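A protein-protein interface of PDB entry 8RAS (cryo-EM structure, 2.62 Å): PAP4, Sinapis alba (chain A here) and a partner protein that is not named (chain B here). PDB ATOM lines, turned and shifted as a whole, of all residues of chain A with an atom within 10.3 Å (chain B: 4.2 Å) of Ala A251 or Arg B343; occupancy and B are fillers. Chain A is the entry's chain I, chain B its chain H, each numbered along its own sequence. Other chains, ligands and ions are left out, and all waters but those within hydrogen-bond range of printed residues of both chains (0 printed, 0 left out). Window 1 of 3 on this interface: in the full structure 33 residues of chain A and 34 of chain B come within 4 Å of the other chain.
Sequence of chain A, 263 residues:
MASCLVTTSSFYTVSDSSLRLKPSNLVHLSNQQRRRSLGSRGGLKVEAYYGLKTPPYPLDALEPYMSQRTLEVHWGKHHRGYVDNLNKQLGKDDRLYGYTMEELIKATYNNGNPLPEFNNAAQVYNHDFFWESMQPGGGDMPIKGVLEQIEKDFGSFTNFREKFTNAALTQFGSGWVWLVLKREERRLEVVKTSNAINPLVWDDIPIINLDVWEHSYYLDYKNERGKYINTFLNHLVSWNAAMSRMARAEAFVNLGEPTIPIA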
ATOM      1  N   LEU A 181     -23.692 -17.752  -2.542  1.00  0.00           N
ATOM      2  CA  LEU A 181     -24.045 -19.109  -2.144  1.00  0.00           C
ATOM      3  C   LEU A 181     -23.804 -19.234  -0.646  1.00  0.00           C
ATOM      4  O   LEU A 181     -22.656 -19.181  -0.191  1.00  0.00           O
ATOM      5  CB  LEU A 181     -23.223 -20.133  -2.922  1.00  0.00           C
ATOM      6  CG  LEU A 181     -23.755 -21.564  -2.971  1.00  0.00           C
ATOM      7  CD1 LEU A 181     -25.113 -21.607  -3.646  1.00  0.00           C
ATOM      8  CD2 LEU A 181     -22.766 -22.466  -3.685  1.00  0.00           C
ATOM      9  N   ARG A 183     -23.046 -20.809   2.719  1.00  0.00           N
ATOM     10  CA  ARG A 183     -22.295 -22.017   3.044  1.00  0.00           C
ATOM     11  C   ARG A 183     -23.105 -22.946   3.941  1.00  0.00           C
ATOM     12  O   ARG A 183     -23.203 -24.150   3.676  1.00  0.00           O
ATOM     13  CB  ARG A 183     -20.972 -21.638   3.707  1.00  0.00           C
ATOM     14  CG  ARG A 183     -19.929 -22.735   3.699  1.00  0.00           C
ATOM     15  CD  ARG A 183     -18.654 -22.260   4.370  1.00  0.00           C
ATOM     16  NE  ARG A 183     -17.946 -21.281   3.555  1.00  0.00           N
ATOM     17  CZ  ARG A 183     -16.849 -21.538   2.858  1.00  0.00           C
ATOM     18  NH1 ARG A 183     -16.298 -22.740   2.855  1.00  0.00           N
ATOM     19  NH2 ARG A 183     -16.291 -20.565   2.145  1.00  0.00           N
ATOM     20  N   ILE A 205     -19.616 -17.521  -0.671  1.00  0.00           N
ATOM     21  CA  ILE A 205     -18.898 -17.472  -1.942  1.00  0.00           C
ATOM     22  C   ILE A 205     -19.722 -16.629  -2.913  1.00  0.00           C
ATOM     23  O   ILE A 205     -20.837 -17.038  -3.274  1.00  0.00           O
ATOM     24  CB  ILE A 205     -18.649 -18.876  -2.502  1.00  0.00           C
ATOM     25  CG1 ILE A 205     -17.894 -19.728  -1.479  1.00  0.00           C
ATOM     26  CG2 ILE A 205     -17.872 -18.797  -3.807  1.00  0.00           C
ATOM     27  CD1 ILE A 205     -18.735 -20.805  -0.844  1.00  0.00           C
ATOM     28  N   ILE A 207     -21.013 -15.150  -6.475  1.00  0.00           N
ATOM     29  CA  ILE A 207     -21.183 -15.730  -7.803  1.00  0.00           C
ATOM     30  C   ILE A 207     -21.257 -14.652  -8.878  1.00  0.00           C
ATOM     31  O   ILE A 207     -20.540 -14.709  -9.881  1.00  0.00           O
ATOM     32  CB  ILE A 207     -22.425 -16.647  -7.863  1.00  0.00           C
ATOM     33  CG1 ILE A 207     -22.442 -17.609  -6.673  1.00  0.00           C
ATOM     34  CG2 ILE A 207     -22.453 -17.421  -9.165  1.00  0.00           C
ATOM     35  CD1 ILE A 207     -21.304 -18.605  -6.675  1.00  0.00           C
ATOM     36  N   MET A 243     -20.702 -20.143 -13.931  1.00  0.00           N
ATOM     37  CA  MET A 243     -20.522 -21.587 -14.030  1.00  0.00           C
ATOM     38  C   MET A 243     -19.376 -22.062 -13.149  1.00  0.00           C
ATOM     39  O   MET A 243     -19.546 -22.957 -12.313  1.00  0.00           O
ATOM     40  CB  MET A 243     -20.256 -21.977 -15.482  1.00  0.00           C
ATOM     41  CG  MET A 243     -21.483 -22.036 -16.349  1.00  0.00           C
ATOM     42  SD  MET A 243     -22.844 -22.809 -15.473  1.00  0.00           S
ATOM     43  CE  MET A 243     -23.487 -23.822 -16.790  1.00  0.00           C
ATOM     44  N   SER A 244     -18.197 -21.461 -13.315  1.00  0.00           N
ATOM     45  CA  SER A 244     -17.019 -21.926 -12.596  1.00  0.00           C
ATOM     46  C   SER A 244     -17.017 -21.473 -11.146  1.00  0.00           C
ATOM     47  O   SER A 244     -16.507 -22.193 -10.279  1.00  0.00           O
ATOM     48  CB  SER A 244     -15.754 -21.442 -13.300  1.00  0.00           C
ATOM     49  OG  SER A 244     -15.868 -21.593 -14.704  1.00  0.00           O
ATOM     50  N   ARG A 245     -17.565 -20.289 -10.863  1.00  0.00           N
ATOM     51  CA  ARG A 245     -17.655 -19.835  -9.481  1.00  0.00           C
ATOM     52  C   ARG A 245     -18.527 -20.770  -8.657  1.00  0.00           C
ATOM     53  O   ARG A 245     -18.189 -21.102  -7.516  1.00  0.00           O
ATOM     54  CB  ARG A 245     -18.200 -18.410  -9.429  1.00  0.00           C
ATOM     55  CG  ARG A 245     -17.155 -17.345  -9.681  1.00  0.00           C
ATOM     56  CD  ARG A 245     -17.759 -16.162 -10.404  1.00  0.00           C
ATOM     57  NE  ARG A 245     -16.771 -15.128 -10.684  1.00  0.00           N
ATOM     58  CZ  ARG A 245     -17.072 -13.874 -10.987  1.00  0.00           C
ATOM     59  NH1 ARG A 245     -18.327 -13.462 -11.060  1.00  0.00           N
ATOM     60  NH2 ARG A 245     -16.089 -13.010 -11.217  1.00  0.00           N
ATOM     61  N   MET A 246     -19.651 -21.209  -9.221  1.00  0.00           N
ATOM     62  CA  MET A 246     -20.473 -22.202  -8.547  1.00  0.00           C
ATOM     63  C   MET A 246     -19.886 -23.601  -8.666  1.00  0.00           C
ATOM     64  O   MET A 246     -20.247 -24.479  -7.877  1.00  0.00           O
ATOM     65  CB  MET A 246     -21.900 -22.166  -9.100  1.00  0.00           C
ATOM     66  CG  MET A 246     -22.919 -21.647  -8.093  1.00  0.00           C
ATOM     67  SD  MET A 246     -24.640 -21.903  -8.559  1.00  0.00           S
ATOM     68  CE  MET A 246     -24.646 -23.656  -8.900  1.00  0.00           C
ATOM     69  N   ALA A 247     -18.994 -23.827  -9.633  1.00  0.00           N
ATOM     70  CA  ALA A 247     -18.219 -25.063  -9.668  1.00  0.00           C
ATOM     71  C   ALA A 247     -17.107 -25.047  -8.630  1.00  0.00           C
ATOM     72  O   ALA A 247     -16.843 -26.064  -7.980  1.00  0.00           O
ATOM     73  CB  ALA A 247     -17.631 -25.283 -11.061  1.00  0.00           C
ATOM     74  N   ARG A 248     -16.434 -23.905  -8.474  1.00  0.00           N
ATOM     75  CA  ARG A 248     -15.416 -23.777  -7.439  1.00  0.00           C
ATOM     76  C   ARG A 248     -16.035 -23.868  -6.051  1.00  0.00           C
ATOM     77  O   ARG A 248     -15.451 -24.466  -5.142  1.00  0.00           O
ATOM     78  CB  ARG A 248     -14.660 -22.461  -7.610  1.00  0.00           C
ATOM     79  CG  ARG A 248     -13.538 -22.251  -6.613  1.00  0.00           C
ATOM     80  CD  ARG A 248     -12.236 -22.839  -7.117  1.00  0.00           C
ATOM     81  NE  ARG A 248     -11.203 -22.827  -6.089  1.00  0.00           N
ATOM     82  CZ  ARG A 248     -10.627 -23.914  -5.593  1.00  0.00           C
ATOM     83  NH1 ARG A 248     -10.960 -25.123  -6.011  1.00  0.00           N
ATOM     84  NH2 ARG A 248      -9.697 -23.782  -4.652  1.00  0.00           N
ATOM     85  N   ALA A 249     -17.219 -23.277  -5.873  1.00  0.00           N
ATOM     86  CA  ALA A 249     -17.922 -23.371  -4.601  1.00  0.00           C
ATOM     87  C   ALA A 249     -18.356 -24.796  -4.283  1.00  0.00           C
ATOM     88  O   ALA A 249     -18.539 -25.124  -3.107  1.00  0.00           O
ATOM     89  CB  ALA A 249     -19.138 -22.445  -4.604  1.00  0.00           C
ATOM     90  N   GLU A 250     -18.524 -25.645  -5.300  1.00  0.00           N
ATOM     91  CA  GLU A 250     -18.891 -27.036  -5.057  1.00  0.00           C
ATOM     92  C   GLU A 250     -17.823 -27.785  -4.274  1.00  0.00           C
ATOM     93  O   GLU A 250     -18.126 -28.815  -3.661  1.00  0.00           O
ATOM     94  CB  GLU A 250     -19.156 -27.752  -6.382  1.00  0.00           C
ATOM     95  CG  GLU A 250     -20.534 -27.495  -6.955  1.00  0.00           C
ATOM     96  CD  GLU A 250     -21.636 -28.098  -6.111  1.00  0.00           C
ATOM     97  OE1 GLU A 250     -21.575 -29.314  -5.831  1.00  0.00           O
ATOM     98  OE2 GLU A 250     -22.563 -27.357  -5.729  1.00  0.00           O
ATOM     99  N   ALA A 251     -16.582 -27.299  -4.284  1.00  0.00           N
ATOM    100  CA  ALA A 251     -15.541 -27.883  -3.453  1.00  0.00           C
ATOM    101  C   ALA A 251     -15.734 -27.581  -1.974  1.00  0.00           C
ATOM    102  O   ALA A 251     -15.023 -28.159  -1.145  1.00  0.00           O
ATOM    103  CB  ALA A 251     -14.166 -27.390  -3.907  1.00  0.00           C
ATOM    104  N   PHE A 252     -16.671 -26.696  -1.624  1.00  0.00           N
ATOM    105  CA  PHE A 252     -16.881 -26.308  -0.239  1.00  0.00           C
ATOM    106  C   PHE A 252     -18.332 -26.349   0.218  1.00  0.00           C
ATOM    107  O   PHE A 252     -18.570 -26.284   1.428  1.00  0.00           O
ATOM    108  CB  PHE A 252     -16.336 -24.892   0.010  1.00  0.00           C
ATOM    109  CG  PHE A 252     -14.956 -24.667  -0.540  1.00  0.00           C
ATOM    110  CD1 PHE A 252     -13.865 -25.323   0.001  1.00  0.00           C
ATOM    111  CD2 PHE A 252     -14.753 -23.798  -1.598  1.00  0.00           C
ATOM    112  CE1 PHE A 252     -12.594 -25.117  -0.505  1.00  0.00           C
ATOM    113  CE2 PHE A 252     -13.486 -23.589  -2.108  1.00  0.00           C
ATOM    114  CZ  PHE A 252     -12.406 -24.250  -1.560  1.00  0.00           C
ATOM    115  N   VAL A 253     -19.306 -26.453  -0.691  1.00  0.00           N
ATOM    116  CA  VAL A 253     -20.716 -26.367  -0.336  1.00  0.00           C
ATOM    117  C   VAL A 253     -21.464 -27.663  -0.625  1.00  0.00           C
ATOM    118  O   VAL A 253     -22.260 -28.117   0.205  1.00  0.00           O
ATOM    119  CB  VAL A 253     -21.402 -25.180  -1.045  1.00  0.00           C
ATOM    120  CG1 VAL A 253     -22.786 -24.955  -0.471  1.00  0.00           C
ATOM    121  CG2 VAL A 253     -20.563 -23.927  -0.901  1.00  0.00           C
ATOM    122  N   ASN A 254     -21.230 -28.274  -1.788  1.00  0.00           N
ATOM    123  CA  ASN A 254     -21.850 -29.546  -2.165  1.00  0.00           C
ATOM    124  C   ASN A 254     -23.379 -29.436  -2.171  1.00  0.00           C
ATOM    125  O   ASN A 254     -24.085 -30.020  -1.347  1.00  0.00           O
ATOM    126  CB  ASN A 254     -21.381 -30.679  -1.244  1.00  0.00           C
ATOM    127  CG  ASN A 254     -21.634 -32.053  -1.835  1.00  0.00           C
ATOM    128  OD1 ASN A 254     -22.760 -32.392  -2.191  1.00  0.00           O
ATOM    129  ND2 ASN A 254     -20.581 -32.852  -1.939  1.00  0.00           N
ATOM    130  N   LEU A 255     -23.872 -28.649  -3.127  1.00  0.00           N
ATOM    131  CA  LEU A 255     -25.307 -28.410  -3.303  1.00  0.00           C
ATOM    132  C   LEU A 255     -26.089 -29.649  -3.760  1.00  0.00           C
ATOM    133  O   LEU A 255     -27.292 -29.506  -4.009  1.00  0.00           O
ATOM    134  CB  LEU A 255     -25.529 -27.277  -4.307  1.00  0.00           C
ATOM    135  CG  LEU A 255     -24.921 -25.914  -3.982  1.00  0.00           C
ATOM    136  CD1 LEU A 255     -24.949 -25.022  -5.210  1.00  0.00           C
ATOM    137  CD2 LEU A 255     -25.656 -25.262  -2.828  1.00  0.00           C
ATOM    138  N   GLY A 256     -25.498 -30.834  -3.886  1.00  0.00           N
ATOM    139  CA  GLY A 256     -26.217 -32.003  -4.347  1.00  0.00           C
ATOM    140  C   GLY A 256     -26.941 -32.725  -3.228  1.00  0.00           C
ATOM    141  O   GLY A 256     -27.219 -32.169  -2.164  1.00  0.00           O
ATOM    142  N   VAL B 325      -3.213 -33.120  -4.935  1.00  0.00           N
ATOM    143  CA  VAL B 325      -3.912 -32.353  -3.914  1.00  0.00           C
ATOM    144  C   VAL B 325      -3.515 -30.888  -4.015  1.00  0.00           C
ATOM    145  O   VAL B 325      -2.410 -30.549  -4.449  1.00  0.00           O
ATOM    146  CB  VAL B 325      -3.624 -32.891  -2.495  1.00  0.00           C
ATOM    147  CG1 VAL B 325      -4.233 -34.271  -2.318  1.00  0.00           C
ATOM    148  CG2 VAL B 325      -2.129 -32.926  -2.235  1.00  0.00           C
ATOM    149  N   GLU B 326      -4.433 -30.017  -3.610  1.00  0.00           N
ATOM    150  CA  GLU B 326      -4.207 -28.580  -3.569  1.00  0.00           C
ATOM    151  C   GLU B 326      -4.277 -28.104  -2.127  1.00  0.00           C
ATOM    152  O   GLU B 326      -5.241 -28.404  -1.416  1.00  0.00           O
ATOM    153  CB  GLU B 326      -5.240 -27.836  -4.416  1.00  0.00           C
ATOM    154  CG  GLU B 326      -5.139 -26.325  -4.320  1.00  0.00           C
ATOM    155  CD  GLU B 326      -6.494 -25.660  -4.166  1.00  0.00           C
ATOM    156  OE1 GLU B 326      -7.495 -26.222  -4.658  1.00  0.00           O
ATOM    157  OE2 GLU B 326      -6.557 -24.576  -3.549  1.00  0.00           O
ATOM    158  N   THR B 328      -5.236 -25.902   0.657  1.00  0.00           N
ATOM    159  CA  THR B 328      -6.271 -24.902   0.876  1.00  0.00           C
ATOM    160  C   THR B 328      -5.913 -23.932   1.992  1.00  0.00           C
ATOM    161  O   THR B 328      -6.221 -22.739   1.888  1.00  0.00           O
ATOM    162  CB  THR B 328      -7.606 -25.586   1.190  1.00  0.00           C
ATOM    163  OG1 THR B 328      -7.986 -26.419   0.090  1.00  0.00           O
ATOM    164  CG2 THR B 328      -8.700 -24.556   1.431  1.00  0.00           C
ATOM    165  N   LEU B 342      -5.796 -29.763   2.825  1.00  0.00           N
ATOM    166  CA  LEU B 342      -5.790 -29.978   1.387  1.00  0.00           C
ATOM    167  C   LEU B 342      -7.190 -30.330   0.895  1.00  0.00           C
ATOM    168  O   LEU B 342      -8.134 -30.482   1.671  1.00  0.00           O
ATOM    169  CB  LEU B 342      -4.809 -31.088   1.000  1.00  0.00           C
ATOM    170  CG  LEU B 342      -3.489 -31.219   1.754  1.00  0.00           C
ATOM    171  CD1 LEU B 342      -2.914 -32.602   1.525  1.00  0.00           C
ATOM    172  CD2 LEU B 342      -2.509 -30.155   1.314  1.00  0.00           C
ATOM    173  N   ARG B 343      -7.303 -30.447  -0.425  1.00  0.00           N
ATOM    174  CA  ARG B 343      -8.468 -31.018  -1.079  1.00  0.00           C
ATOM    175  C   ARG B 343      -7.982 -31.880  -2.233  1.00  0.00           C
ATOM    176  O   ARG B 343      -6.913 -31.637  -2.797  1.00  0.00           O
ATOM    177  CB  ARG B 343      -9.434 -29.941  -1.588  1.00  0.00           C
ATOM    178  CG  ARG B 343      -8.870 -29.064  -2.689  1.00  0.00           C
ATOM    179  CD  ARG B 343      -9.964 -28.232  -3.334  1.00  0.00           C
ATOM    180  NE  ARG B 343     -10.870 -29.051  -4.130  1.00  0.00           N
ATOM    181  CZ  ARG B 343     -10.723 -29.290  -5.425  1.00  0.00           C
ATOM    182  NH1 ARG B 343      -9.711 -28.786  -6.110  1.00  0.00           N
ATOM    183  NH2 ARG B 343     -11.613 -30.056  -6.048  1.00  0.00           N
ATOM    184  N   PHE B 344      -8.769 -32.894  -2.575  1.00  0.00           N
ATOM    185  CA  PHE B 344      -8.377 -33.831  -3.620  1.00  0.00           C
ATOM    186  C   PHE B 344      -8.639 -33.220  -4.990  1.00  0.00           C
ATOM    187  O   PHE B 344      -9.786 -32.912  -5.331  1.00  0.00           O
ATOM    188  CB  PHE B 344      -9.131 -35.150  -3.466  1.00  0.00           C
ATOM    189  CG  PHE B 344      -8.592 -36.032  -2.381  1.00  0.00           C
ATOM    190  CD1 PHE B 344      -7.252 -36.376  -2.353  1.00  0.00           C
ATOM    191  CD2 PHE B 344      -9.424 -36.525  -1.393  1.00  0.00           C
ATOM    192  CE1 PHE B 344      -6.752 -37.190  -1.358  1.00  0.00           C
ATOM    193  CE2 PHE B 344      -8.930 -37.341  -0.396  1.00  0.00           C
ATOM    194  CZ  PHE B 344      -7.593 -37.672  -0.379  1.00  0.00           C
ATOM    195  N   VAL B 345      -7.576 -33.044  -5.773  1.00  0.00           N
ATOM    196  CA  VAL B 345      -7.735 -32.603  -7.154  1.00  0.00           C
ATOM    197  C   VAL B 345      -8.004 -33.796  -8.062  1.00  0.00           C
ATOM    198  O   VAL B 345      -8.959 -33.796  -8.846  1.00  0.00           O
ATOM    199  CB  VAL B 345      -6.495 -31.813  -7.610  1.00  0.00           C
ATOM    200  CG1 VAL B 345      -6.698 -31.271  -9.014  1.00  0.00           C
ATOM    201  CG2 VAL B 345      -6.196 -30.687  -6.634  1.00  0.00           C
ATOM    202  N   ASN B 348     -11.523 -36.489  -8.068  1.00  0.00           N
ATOM    203  CA  ASN B 348     -12.433 -35.456  -7.589  1.00  0.00           C
ATOM    204  C   ASN B 348     -13.572 -36.125  -6.829  1.00  0.00           C
ATOM    205  O   ASN B 348     -14.365 -36.870  -7.415  1.00  0.00           O
ATOM    206  CB  ASN B 348     -12.963 -34.628  -8.756  1.00  0.00           C
ATOM    207  CG  ASN B 348     -13.637 -33.351  -8.308  1.00  0.00           C
ATOM    208  OD1 ASN B 348     -14.830 -33.338  -8.009  1.00  0.00           O
ATOM    209  ND2 ASN B 348     -12.876 -32.264  -8.267  1.00  0.00           N
ATOM    210  N   ASP B 350     -15.500 -34.145  -4.651  1.00  0.00           N
ATOM    211  CA  ASP B 350     -16.226 -33.012  -4.087  1.00  0.00           C
ATOM    212  C   ASP B 350     -17.718 -33.299  -4.004  1.00  0.00           C
ATOM    213  O   ASP B 350     -18.386 -32.885  -3.050  1.00  0.00           O
ATOM    214  CB  ASP B 350     -15.967 -31.757  -4.919  1.00  0.00           C
ATOM    215  CG  ASP B 350     -14.565 -31.216  -4.735  1.00  0.00           C
ATOM    216  OD1 ASP B 350     -13.885 -31.636  -3.776  1.00  0.00           O
ATOM    217  OD2 ASP B 350     -14.143 -30.368  -5.548  1.00  0.00           O
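NH2 of Arg A248 lies within salt-bridge range of OE1 of Glu B326 (3.3 Å). The backbone carbonyl oxygen (O) of Asp B350 is in hydrogen-bond range of the side-chain amide nitrogen (ND2) of Asn A254 (2.5 Å).
Ala A251 touches just these residues of chain B: Arg B343 (3.7 Å) and Asp B350 (3.4 Å). Of chain A, only Arg A248 and Ala A251 come within 4 Å of Arg B343. Val B325 touches none of the printed residues of chain A. Glu B326 touches just one residue of chain A: Arg A248. No residue of chain A comes within 4 Å of Leu B342. No residue of chain A comes within 4 Å of Phe B344. No residue of chain A comes within 4 Å of Val B345. Asp B350 touches just these residues of chain A: Glu A250 (3.9 Å), Ala A251 (3.4 Å) and Asn A254 (2.5 Å). Of the printed residues of chain B, Arg A248 touches Glu B326 and Arg B343. Printed residues of chain B within 4 Å of Glu A250: Asp B350. Of the printed residues of chain B, Asn A254 touches Asp B350 (2.5 Å). The nearest printed residue of chain B that does not touch Ala A251 is Asn B348 (6.7 Å).
NH1 of Arg A248 touches NH1 of Arg B343, 3.9 Å away. CB of Asp B350 touches O of Glu A250 (3.9 Å). Ala A251 touches Arg B343. Ala A251 touches Asp B350.
Of the 18 printed residues of chain A, 4 touch a printed residue of chain B. Hydrophobic or aromatic side chains of chain A within 4 Å of the printed part of chain B: Ala A251.
The side-chain carboxylate of Glu B326 is in salt-bridge range of the guanidinium group of Arg B343 (3.7 Å). The guanidinium group of Arg B343 lies close to the side-chain amide nitrogen of Asn B348, 3.4 Å away. The guanidinium group (NH2) of Arg B343 lies within salt-bridge range of the side-chain carboxylate (OD2) of Asp B350, 2.6 Å away. OE2 of Glu A250 lies within hydrogen-bond range of N of Leu A255 (3.2 Å).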
